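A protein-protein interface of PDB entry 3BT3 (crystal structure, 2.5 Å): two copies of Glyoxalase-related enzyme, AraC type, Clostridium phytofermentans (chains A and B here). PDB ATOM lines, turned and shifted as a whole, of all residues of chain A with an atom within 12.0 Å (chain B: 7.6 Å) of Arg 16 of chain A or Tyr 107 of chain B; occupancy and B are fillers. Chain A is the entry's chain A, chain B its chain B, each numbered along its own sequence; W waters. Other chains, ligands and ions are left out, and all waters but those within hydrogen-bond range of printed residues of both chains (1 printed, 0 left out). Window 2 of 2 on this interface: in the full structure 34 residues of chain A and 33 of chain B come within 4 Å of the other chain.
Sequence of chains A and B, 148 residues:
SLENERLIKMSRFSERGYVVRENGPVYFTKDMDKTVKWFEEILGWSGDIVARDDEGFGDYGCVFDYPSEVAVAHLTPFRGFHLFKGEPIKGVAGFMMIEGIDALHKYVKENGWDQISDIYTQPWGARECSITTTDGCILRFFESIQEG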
ATOM      1  N   GLU A  15       5.130  14.181  26.417  1.00  0.00           N
ATOM      2  CA  GLU A  15       6.313  13.959  25.532  1.00  0.00           C
ATOM      3  C   GLU A  15       6.525  12.473  25.323  1.00  0.00           C
ATOM      4  O   GLU A  15       5.620  11.657  25.535  1.00  0.00           O
ATOM      5  CB  GLU A  15       7.580  14.521  26.171  1.00  0.00           C
ATOM      6  CG  GLU A  15       7.402  15.877  26.780  1.00  0.00           C
ATOM      7  CD  GLU A  15       6.614  15.833  28.049  1.00  0.00           C
ATOM      8  OE1 GLU A  15       7.179  15.421  29.083  1.00  0.00           O
ATOM      9  OE2 GLU A  15       5.424  16.204  28.001  1.00  0.00           O
ATOM     10  N   ARG A  16       7.736  12.135  24.905  1.00  0.00           N
ATOM     11  CA  ARG A  16       8.113  10.753  24.696  1.00  0.00           C
ATOM     12  C   ARG A  16       9.606  10.757  24.471  1.00  0.00           C
ATOM     13  O   ARG A  16      10.090  11.244  23.450  1.00  0.00           O
ATOM     14  CB  ARG A  16       7.390  10.160  23.486  1.00  0.00           C
ATOM     15  CG  ARG A  16       7.165   8.652  23.583  1.00  0.00           C
ATOM     16  CD  ARG A  16       6.363   8.296  24.833  1.00  0.00           C
ATOM     17  NE  ARG A  16       7.178   8.335  26.047  1.00  0.00           N
ATOM     18  CZ  ARG A  16       6.687   8.431  27.280  1.00  0.00           C
ATOM     19  NH1 ARG A  16       5.376   8.504  27.474  1.00  0.00           N
ATOM     20  NH2 ARG A  16       7.509   8.443  28.322  1.00  0.00           N
ATOM     21  N   GLY A  17      10.332  10.245  25.455  1.00  0.00           N
ATOM     22  CA  GLY A  17      11.771  10.186  25.351  1.00  0.00           C
ATOM     23  C   GLY A  17      12.479  11.327  26.047  1.00  0.00           C
ATOM     24  O   GLY A  17      13.709  11.324  26.112  1.00  0.00           O
ATOM     25  N   TYR A  18      11.735  12.299  26.572  1.00  0.00           N
ATOM     26  CA  TYR A  18      12.380  13.421  27.246  1.00  0.00           C
ATOM     27  C   TYR A  18      11.549  14.068  28.359  1.00  0.00           C
ATOM     28  O   TYR A  18      10.324  14.114  28.290  1.00  0.00           O
ATOM     29  CB  TYR A  18      12.769  14.482  26.217  1.00  0.00           C
ATOM     30  CG  TYR A  18      11.676  15.475  25.927  1.00  0.00           C
ATOM     31  CD1 TYR A  18      11.508  16.603  26.731  1.00  0.00           C
ATOM     32  CD2 TYR A  18      10.802  15.284  24.856  1.00  0.00           C
ATOM     33  CE1 TYR A  18      10.499  17.518  26.478  1.00  0.00           C
ATOM     34  CE2 TYR A  18       9.783  16.198  24.592  1.00  0.00           C
ATOM     35  CZ  TYR A  18       9.638  17.310  25.410  1.00  0.00           C
ATOM     36  OH  TYR A  18       8.620  18.197  25.183  1.00  0.00           O
ATOM     37  N   VAL A  19      12.237  14.585  29.375  1.00  0.00           N
ATOM     38  CA  VAL A  19      11.578  15.229  30.504  1.00  0.00           C
ATOM     39  C   VAL A  19      12.161  16.601  30.763  1.00  0.00           C
ATOM     40  O   VAL A  19      13.348  16.831  30.535  1.00  0.00           O
ATOM     41  CB  VAL A  19      11.743  14.419  31.809  1.00  0.00           C
ATOM     42  CG1 VAL A  19      11.220  13.011  31.620  1.00  0.00           C
ATOM     43  CG2 VAL A  19      13.207  14.398  32.225  1.00  0.00           C
ATOM     44  N   VAL A  20      11.326  17.511  31.246  1.00  0.00           N
ATOM     45  CA  VAL A  20      11.795  18.847  31.556  1.00  0.00           C
ATOM     46  C   VAL A  20      12.291  18.815  32.990  1.00  0.00           C
ATOM     47  O   VAL A  20      11.516  18.596  33.915  1.00  0.00           O
ATOM     48  CB  VAL A  20      10.667  19.894  31.413  1.00  0.00           C
ATOM     49  CG1 VAL A  20      11.162  21.266  31.871  1.00  0.00           C
ATOM     50  CG2 VAL A  20      10.202  19.960  29.971  1.00  0.00           C
ATOM     51  N   ARG A  21      13.588  19.013  33.177  1.00  0.00           N
ATOM     52  CA  ARG A  21      14.159  18.992  34.513  1.00  0.00           C
ATOM     53  C   ARG A  21      13.973  20.325  35.228  1.00  0.00           C
ATOM     54  O   ARG A  21      13.602  20.359  36.402  1.00  0.00           O
ATOM     55  CB  ARG A  21      15.643  18.641  34.437  1.00  0.00           C
ATOM     56  CG  ARG A  21      16.033  17.403  35.229  1.00  0.00           C
ATOM     57  CD  ARG A  21      15.080  16.243  34.959  1.00  0.00           C
ATOM     58  NE  ARG A  21      15.565  14.979  35.515  1.00  0.00           N
ATOM     59  CZ  ARG A  21      14.837  13.869  35.599  1.00  0.00           C
ATOM     60  NH1 ARG A  21      13.582  13.858  35.169  1.00  0.00           N
ATOM     61  NH2 ARG A  21      15.366  12.761  36.102  1.00  0.00           N
ATOM     62  N   PHE B  39       1.441  23.262  21.760  1.00  0.00           N
ATOM     63  CA  PHE B  39       2.186  22.662  22.857  1.00  0.00           C
ATOM     64  C   PHE B  39       1.861  21.184  22.993  1.00  0.00           C
ATOM     65  O   PHE B  39       2.753  20.360  23.217  1.00  0.00           O
ATOM     66  CB  PHE B  39       1.868  23.389  24.168  1.00  0.00           C
ATOM     67  CG  PHE B  39       2.845  24.475  24.511  1.00  0.00           C
ATOM     68  CD1 PHE B  39       4.018  24.173  25.195  1.00  0.00           C
ATOM     69  CD2 PHE B  39       2.604  25.796  24.139  1.00  0.00           C
ATOM     70  CE1 PHE B  39       4.932  25.164  25.508  1.00  0.00           C
ATOM     71  CE2 PHE B  39       3.513  26.798  24.446  1.00  0.00           C
ATOM     72  CZ  PHE B  39       4.681  26.485  25.131  1.00  0.00           C
ATOM     73  N   GLU B  40       0.583  20.846  22.859  1.00  0.00           N
ATOM     74  CA  GLU B  40       0.162  19.457  22.984  1.00  0.00           C
ATOM     75  C   GLU B  40       0.544  18.617  21.755  1.00  0.00           C
ATOM     76  O   GLU B  40       1.018  17.496  21.892  1.00  0.00           O
ATOM     77  CB  GLU B  40      -1.357  19.381  23.230  1.00  0.00           C
ATOM     78  CG  GLU B  40      -1.834  20.194  24.441  1.00  0.00           C
ATOM     79  CD  GLU B  40      -3.314  19.988  24.781  1.00  0.00           C
ATOM     80  OE1 GLU B  40      -4.167  20.111  23.875  1.00  0.00           O
ATOM     81  OE2 GLU B  40      -3.628  19.716  25.966  1.00  0.00           O
ATOM     82  N   GLU B  41       0.376  19.169  20.560  1.00  0.00           N
ATOM     83  CA  GLU B  41       0.674  18.420  19.346  1.00  0.00           C
ATOM     84  C   GLU B  41       2.128  18.356  18.892  1.00  0.00           C
ATOM     85  O   GLU B  41       2.542  17.361  18.300  1.00  0.00           O
ATOM     86  CB  GLU B  41      -0.195  18.939  18.203  1.00  0.00           C
ATOM     87  CG  GLU B  41      -1.662  18.615  18.401  1.00  0.00           C
ATOM     88  CD  GLU B  41      -2.551  19.153  17.301  1.00  0.00           C
ATOM     89  OE1 GLU B  41      -3.741  18.771  17.268  1.00  0.00           O
ATOM     90  OE2 GLU B  41      -2.071  19.962  16.475  1.00  0.00           O
ATOM     91  N   ILE B  42       2.903  19.400  19.169  1.00  0.00           N
ATOM     92  CA  ILE B  42       4.296  19.428  18.749  1.00  0.00           C
ATOM     93  C   ILE B  42       5.299  19.003  19.814  1.00  0.00           C
ATOM     94  O   ILE B  42       6.260  18.300  19.508  1.00  0.00           O
ATOM     95  CB  ILE B  42       4.686  20.823  18.262  1.00  0.00           C
ATOM     96  CG1 ILE B  42       3.699  21.289  17.193  1.00  0.00           C
ATOM     97  CG2 ILE B  42       6.112  20.800  17.722  1.00  0.00           C
ATOM     98  CD1 ILE B  42       3.589  20.350  16.025  1.00  0.00           C
ATOM     99  N   LEU B  43       5.080  19.432  21.056  1.00  0.00           N
ATOM    100  CA  LEU B  43       5.985  19.104  22.156  1.00  0.00           C
ATOM    101  C   LEU B  43       5.485  17.983  23.059  1.00  0.00           C
ATOM    102  O   LEU B  43       6.240  17.466  23.890  1.00  0.00           O
ATOM    103  CB  LEU B  43       6.243  20.342  23.019  1.00  0.00           C
ATOM    104  CG  LEU B  43       6.966  21.523  22.377  1.00  0.00           C
ATOM    105  CD1 LEU B  43       7.148  22.619  23.415  1.00  0.00           C
ATOM    106  CD2 LEU B  43       8.320  21.066  21.834  1.00  0.00           C
ATOM    107  N   GLY B  44       4.211  17.625  22.915  1.00  0.00           N
ATOM    108  CA  GLY B  44       3.660  16.562  23.735  1.00  0.00           C
ATOM    109  C   GLY B  44       3.351  16.968  25.167  1.00  0.00           C
ATOM    110  O   GLY B  44       3.374  16.129  26.066  1.00  0.00           O
ATOM    111  N   TRP B  45       3.070  18.250  25.389  1.00  0.00           N
ATOM    112  CA  TRP B  45       2.732  18.733  26.723  1.00  0.00           C
ATOM    113  C   TRP B  45       1.217  18.675  26.919  1.00  0.00           C
ATOM    114  O   TRP B  45       0.490  18.227  26.038  1.00  0.00           O
ATOM    115  CB  TRP B  45       3.203  20.176  26.892  1.00  0.00           C
ATOM    116  CG  TRP B  45       4.680  20.323  27.002  1.00  0.00           C
ATOM    117  CD1 TRP B  45       5.630  19.517  26.443  1.00  0.00           C
ATOM    118  CD2 TRP B  45       5.388  21.371  27.673  1.00  0.00           C
ATOM    119  NE1 TRP B  45       6.881  19.999  26.722  1.00  0.00           N
ATOM    120  CE2 TRP B  45       6.765  21.137  27.476  1.00  0.00           C
ATOM    121  CE3 TRP B  45       4.992  22.484  28.427  1.00  0.00           C
ATOM    122  CZ2 TRP B  45       7.756  21.981  28.000  1.00  0.00           C
ATOM    123  CZ3 TRP B  45       5.971  23.320  28.948  1.00  0.00           C
ATOM    124  CH2 TRP B  45       7.343  23.061  28.732  1.00  0.00           C
ATOM    125  N   GLY B 100      17.204  14.046  27.462  1.00  0.00           N
ATOM    126  CA  GLY B 100      16.689  13.413  26.262  1.00  0.00           C
ATOM    127  C   GLY B 100      16.482  14.408  25.135  1.00  0.00           C
ATOM    128  O   GLY B 100      15.449  14.381  24.461  1.00  0.00           O
ATOM    129  N   ILE B 101      17.464  15.280  24.917  1.00  0.00           N
ATOM    130  CA  ILE B 101      17.371  16.286  23.865  1.00  0.00           C
ATOM    131  C   ILE B 101      17.224  15.648  22.488  1.00  0.00           C
ATOM    132  O   ILE B 101      16.451  16.124  21.659  1.00  0.00           O
ATOM    133  CB  ILE B 101      18.600  17.224  23.857  1.00  0.00           C
ATOM    134  CG1 ILE B 101      18.323  18.403  22.926  1.00  0.00           C
ATOM    135  CG2 ILE B 101      19.851  16.469  23.413  1.00  0.00           C
ATOM    136  CD1 ILE B 101      19.412  19.438  22.907  1.00  0.00           C
ATOM    137  N   ASP B 102      17.969  14.575  22.246  1.00  0.00           N
ATOM    138  CA  ASP B 102      17.889  13.871  20.975  1.00  0.00           C
ATOM    139  C   ASP B 102      16.445  13.419  20.776  1.00  0.00           C
ATOM    140  O   ASP B 102      15.853  13.630  19.718  1.00  0.00           O
ATOM    141  CB  ASP B 102      18.830  12.670  20.983  1.00  0.00           C
ATOM    142  CG  ASP B 102      20.291  13.079  21.076  1.00  0.00           C
ATOM    143  OD1 ASP B 102      20.784  13.708  20.110  1.00  0.00           O
ATOM    144  OD2 ASP B 102      20.943  12.786  22.110  1.00  0.00           O
ATOM    145  N   ALA B 103      15.873  12.815  21.811  1.00  0.00           N
ATOM    146  CA  ALA B 103      14.491  12.362  21.744  1.00  0.00           C
ATOM    147  C   ALA B 103      13.578  13.550  21.437  1.00  0.00           C
ATOM    148  O   ALA B 103      12.661  13.443  20.617  1.00  0.00           O
ATOM    149  CB  ALA B 103      14.084  11.713  23.069  1.00  0.00           C
ATOM    150  N   LEU B 104      13.832  14.682  22.092  1.00  0.00           N
ATOM    151  CA  LEU B 104      13.022  15.878  21.881  1.00  0.00           C
ATOM    152  C   LEU B 104      12.990  16.287  20.425  1.00  0.00           C
ATOM    153  O   LEU B 104      11.922  16.511  19.854  1.00  0.00           O
ATOM    154  CB  LEU B 104      13.556  17.055  22.692  1.00  0.00           C
ATOM    155  CG  LEU B 104      12.966  18.401  22.242  1.00  0.00           C
ATOM    156  CD1 LEU B 104      11.473  18.439  22.577  1.00  0.00           C
ATOM    157  CD2 LEU B 104      13.695  19.555  22.926  1.00  0.00           C
ATOM    158  N   HIS B 105      14.170  16.395  19.831  1.00  0.00           N
ATOM    159  CA  HIS B 105      14.287  16.801  18.439  1.00  0.00           C
ATOM    160  C   HIS B 105      13.569  15.834  17.505  1.00  0.00           C
ATOM    161  O   HIS B 105      12.933  16.246  16.539  1.00  0.00           O
ATOM    162  CB  HIS B 105      15.764  16.922  18.057  1.00  0.00           C
ATOM    163  CG  HIS B 105      15.984  17.476  16.690  1.00  0.00           C
ATOM    164  ND1 HIS B 105      15.940  16.696  15.556  1.00  0.00           N
ATOM    165  CD2 HIS B 105      16.191  18.746  16.269  1.00  0.00           C
ATOM    166  CE1 HIS B 105      16.108  17.463  14.492  1.00  0.00           C
ATOM    167  NE2 HIS B 105      16.261  18.710  14.899  1.00  0.00           N
ATOM    168  N   LYS B 106      13.655  14.546  17.803  1.00  0.00           N
ATOM    169  CA  LYS B 106      12.987  13.561  16.972  1.00  0.00           C
ATOM    170  C   LYS B 106      11.469  13.704  17.099  1.00  0.00           C
ATOM    171  O   LYS B 106      10.751  13.704  16.098  1.00  0.00           O
ATOM    172  CB  LYS B 106      13.415  12.149  17.378  1.00  0.00           C
ATOM    173  CG  LYS B 106      12.894  11.062  16.456  1.00  0.00           C
ATOM    174  CD  LYS B 106      13.426   9.697  16.873  1.00  0.00           C
ATOM    175  CE  LYS B 106      13.089   8.624  15.849  1.00  0.00           C
ATOM    176  NZ  LYS B 106      13.862   7.370  16.098  1.00  0.00           N
ATOM    177  N   TYR B 107      10.987  13.841  18.330  1.00  0.00           N
ATOM    178  CA  TYR B 107       9.553  13.973  18.566  1.00  0.00           C
ATOM    179  C   TYR B 107       8.979  15.162  17.814  1.00  0.00           C
ATOM    180  O   TYR B 107       8.008  15.023  17.069  1.00  0.00           O
ATOM    181  CB  TYR B 107       9.269  14.140  20.057  1.00  0.00           C
ATOM    182  CG  TYR B 107       7.819  13.943  20.442  1.00  0.00           C
ATOM    183  CD1 TYR B 107       7.259  12.665  20.491  1.00  0.00           C
ATOM    184  CD2 TYR B 107       7.013  15.030  20.798  1.00  0.00           C
ATOM    185  CE1 TYR B 107       5.935  12.465  20.893  1.00  0.00           C
ATOM    186  CE2 TYR B 107       5.682  14.845  21.199  1.00  0.00           C
ATOM    187  CZ  TYR B 107       5.149  13.556  21.248  1.00  0.00           C
ATOM    188  OH  TYR B 107       3.845  13.353  21.654  1.00  0.00           O
ATOM    189  N   VAL B 108       9.583  16.330  18.004  1.00  0.00           N
ATOM    190  CA  VAL B 108       9.104  17.531  17.334  1.00  0.00           C
ATOM    191  C   VAL B 108       9.114  17.344  15.829  1.00  0.00           C
ATOM    192  O   VAL B 108       8.151  17.694  15.147  1.00  0.00           O
ATOM    193  CB  VAL B 108       9.957  18.774  17.702  1.00  0.00           C
ATOM    194  CG1 VAL B 108       9.623  19.934  16.785  1.00  0.00           C
ATOM    195  CG2 VAL B 108       9.702  19.169  19.130  1.00  0.00           C
ATOM    196  N   LYS B 109      10.198  16.773  15.317  1.00  0.00           N
ATOM    197  CA  LYS B 109      10.333  16.536  13.881  1.00  0.00           C
ATOM    198  C   LYS B 109       9.257  15.574  13.359  1.00  0.00           C
ATOM    199  O   LYS B 109       8.620  15.838  12.342  1.00  0.00           O
ATOM    200  CB  LYS B 109      11.734  15.992  13.572  1.00  0.00           C
ATOM    201  CG  LYS B 109      12.358  16.618  12.336  1.00  0.00           C
ATOM    202  CD  LYS B 109      12.438  18.130  12.484  1.00  0.00           C
ATOM    203  CE  LYS B 109      12.643  18.818  11.137  1.00  0.00           C
ATOM    204  NZ  LYS B 109      13.994  18.593  10.557  1.00  0.00           N
ATOM    205  N   GLU B 110       9.057  14.462  14.061  1.00  0.00           N
ATOM    206  CA  GLU B 110       8.044  13.487  13.660  1.00  0.00           C
ATOM    207  C   GLU B 110       6.656  14.130  13.619  1.00  0.00           C
ATOM    208  O   GLU B 110       5.838  13.804  12.753  1.00  0.00           O
ATOM    209  CB  GLU B 110       8.012  12.303  14.638  1.00  0.00           C
ATOM    210  CG  GLU B 110       9.167  11.317  14.508  1.00  0.00           C
ATOM    211  CD  GLU B 110       9.254  10.373  15.701  1.00  0.00           C
ATOM    212  OE1 GLU B 110      10.003   9.372  15.628  1.00  0.00           O
ATOM    213  OE2 GLU B 110       8.578  10.635  16.722  1.00  0.00           O
ATOM    214  N   ASN B 111       6.392  15.041  14.555  1.00  0.00           N
ATOM    215  CA  ASN B 111       5.096  15.700  14.611  1.00  0.00           C
ATOM    216  C   ASN B 111       4.880  16.739  13.519  1.00  0.00           C
ATOM    217  O   ASN B 111       3.843  17.406  13.490  1.00  0.00           O
ATOM    218  CB  ASN B 111       4.864  16.305  15.999  1.00  0.00           C
ATOM    219  CG  ASN B 111       4.490  15.254  17.024  1.00  0.00           C
ATOM    220  OD1 ASN B 111       3.499  14.543  16.859  1.00  0.00           O
ATOM    221  ND2 ASN B 111       5.283  15.143  18.087  1.00  0.00           N
ATOM    222  N   GLY B 112       5.859  16.868  12.622  1.00  0.00           N
ATOM    223  CA  GLY B 112       5.737  17.789  11.503  1.00  0.00           C
ATOM    224  C   GLY B 112       6.281  19.200  11.634  1.00  0.00           C
ATOM    225  O   GLY B 112       6.350  19.936  10.639  1.00  0.00           O
ATOM    226  N   TRP B 113       6.670  19.597  12.838  1.00  0.00           N
ATOM    227  CA  TRP B 113       7.198  20.943  13.017  1.00  0.00           C
ATOM    228  C   TRP B 113       8.639  21.013  12.500  1.00  0.00           C
ATOM    229  O   TRP B 113       9.499  20.251  12.933  1.00  0.00           O
ATOM    230  CB  TRP B 113       7.136  21.335  14.492  1.00  0.00           C
ATOM    231  CG  TRP B 113       7.234  22.797  14.697  1.00  0.00           C
ATOM    232  CD1 TRP B 113       8.318  23.501  15.144  1.00  0.00           C
ATOM    233  CD2 TRP B 113       6.211  23.756  14.433  1.00  0.00           C
ATOM    234  NE1 TRP B 113       8.030  24.844  15.175  1.00  0.00           N
ATOM    235  CE2 TRP B 113       6.741  25.027  14.745  1.00  0.00           C
ATOM    236  CE3 TRP B 113       4.895  23.665  13.959  1.00  0.00           C
ATOM    237  CZ2 TRP B 113       5.998  26.199  14.603  1.00  0.00           C
ATOM    238  CZ3 TRP B 113       4.161  24.824  13.815  1.00  0.00           C
ATOM    239  CH2 TRP B 113       4.714  26.080  14.138  1.00  0.00           C
ATOM    240  N   ILE B 116      12.710  24.106  14.067  1.00  0.00           N
ATOM    241  CA  ILE B 116      13.518  23.736  15.211  1.00  0.00           C
ATOM    242  C   ILE B 116      14.932  23.688  14.656  1.00  0.00           C
ATOM    243  O   ILE B 116      15.156  23.183  13.563  1.00  0.00           O
ATOM    244  CB  ILE B 116      13.108  22.348  15.794  1.00  0.00           C
ATOM    245  CG1 ILE B 116      14.122  21.906  16.852  1.00  0.00           C
ATOM    246  CG2 ILE B 116      12.997  21.312  14.678  1.00  0.00           C
ATOM    247  CD1 ILE B 116      13.691  20.722  17.670  1.00  0.00           C
HETATM  248  O   HOH W   1      11.202  10.834  20.681  1.00  0.00           O
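OH of Tyr 18 of chain A sits at hydrogen-bond distance from NE1 of Trp 45 of chain B (2.9 Å). OH of Tyr 18 of chain A lies within hydrogen-bond range of O of Leu 43 of chain B, at 2.8 Å. The backbone NH (N) of Glu 15 of chain A sits at hydrogen-bond distance from the backbone carbonyl oxygen (O) of Gly 44 of chain B, 2.6 Å away.
O of Phe 39 of chain B is in hydrogen-bond range of N of Gly 44 of chain B (3.1 Å). The backbone carbonyl oxygen of Tyr 107 of chain B lies within hydrogen-bond range of the side-chain amide nitrogen of Asn 111 of chain B, 2.9 Å away. The backbone NH (N) of Trp 45 of chain B sits at hydrogen-bond distance from the backbone carbonyl oxygen (O) of Phe 39 of chain B (3.0 Å).
Glu 15 of chain A touches Leu 43 of chain B. Glu 15 of chain A touches Trp 45 of chain B. CB of Arg 16 of chain A touches CE1 of Tyr 107 of chain B, 3.8 Å away. Gly 17 of chain A touches Gly 100 of chain B (O to CA, 3.6 Å). Gly 17 of chain A touches Ala 103 of chain B. Tyr 18 of chain A touches Gly 100 of chain B. CD1 of Leu 104 of chain B touches CE2 of Tyr 18 of chain A, 3.5 Å away. CZ2 of Trp 45 of chain B touches CG2 of Val 20 of chain A, 3.7 Å away.
Printed residues of chain B within 4 Å of Glu 15 of chain A: Leu 43, Gly 44 and Trp 45. Of chain B, only Tyr 107 comes within 4 Å of Arg 16 of chain A. Of the printed residues of chain B, Tyr 18 of chain A touches Leu 43 (2.8 Å), Trp 45 (2.9 Å), Gly 100 (3.2 Å) and Leu 104 (3.5 Å). No residue of chain A comes within 4 Å of Ile 42 of chain B. Gly 44 of chain B touches one residue of chain A. Of the printed residues of chain A, Gly 100 of chain B touches Gly 17 (3.6 Å) and Tyr 18 (3.2 Å). Leu 104 of chain B touches just one residue of chain A: Tyr 18 (3.5 Å). Lys 106 of chain B touches none of the printed residues of chain A. Of chain A, only Arg 16 (3.8 Å) comes within 4 Å of Tyr 107 of chain B. No residue of chain A comes within 4 Å of Val 108 of chain B. No residue of chain A comes within 4 Å of Glu 110 of chain B. The nearest residue of chain A that does not touch Tyr 107 of chain B is Glu 15 of chain A (4.4 Å).
Of the 22 printed residues of chain B, 7 touch a printed residue of chain A. Hydrophobic or aromatic side chains of chain B that line the printed part of chain A: Leu 43, Trp 45, Ala 103, Leu 104 and Tyr 107. Printed residues of chain A that touch a printed residue of chain B: Glu 15, Arg 16, Gly 17, Tyr 18 and Val 20. Hydrophobic or aromatic side chains of chain A that line the printed part of chain B: Tyr 18 and Val 20. Among the printed residues, no Asp or Glu carboxylate lies within 4 Å of a Lys or Arg side-chain nitrogen of the other chain.
No position is printed for both chains.
Water W1 bridges O of Ala 103 of chain B (3.0 Å) and O of Arg 16 of chain A (3.0 Å).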
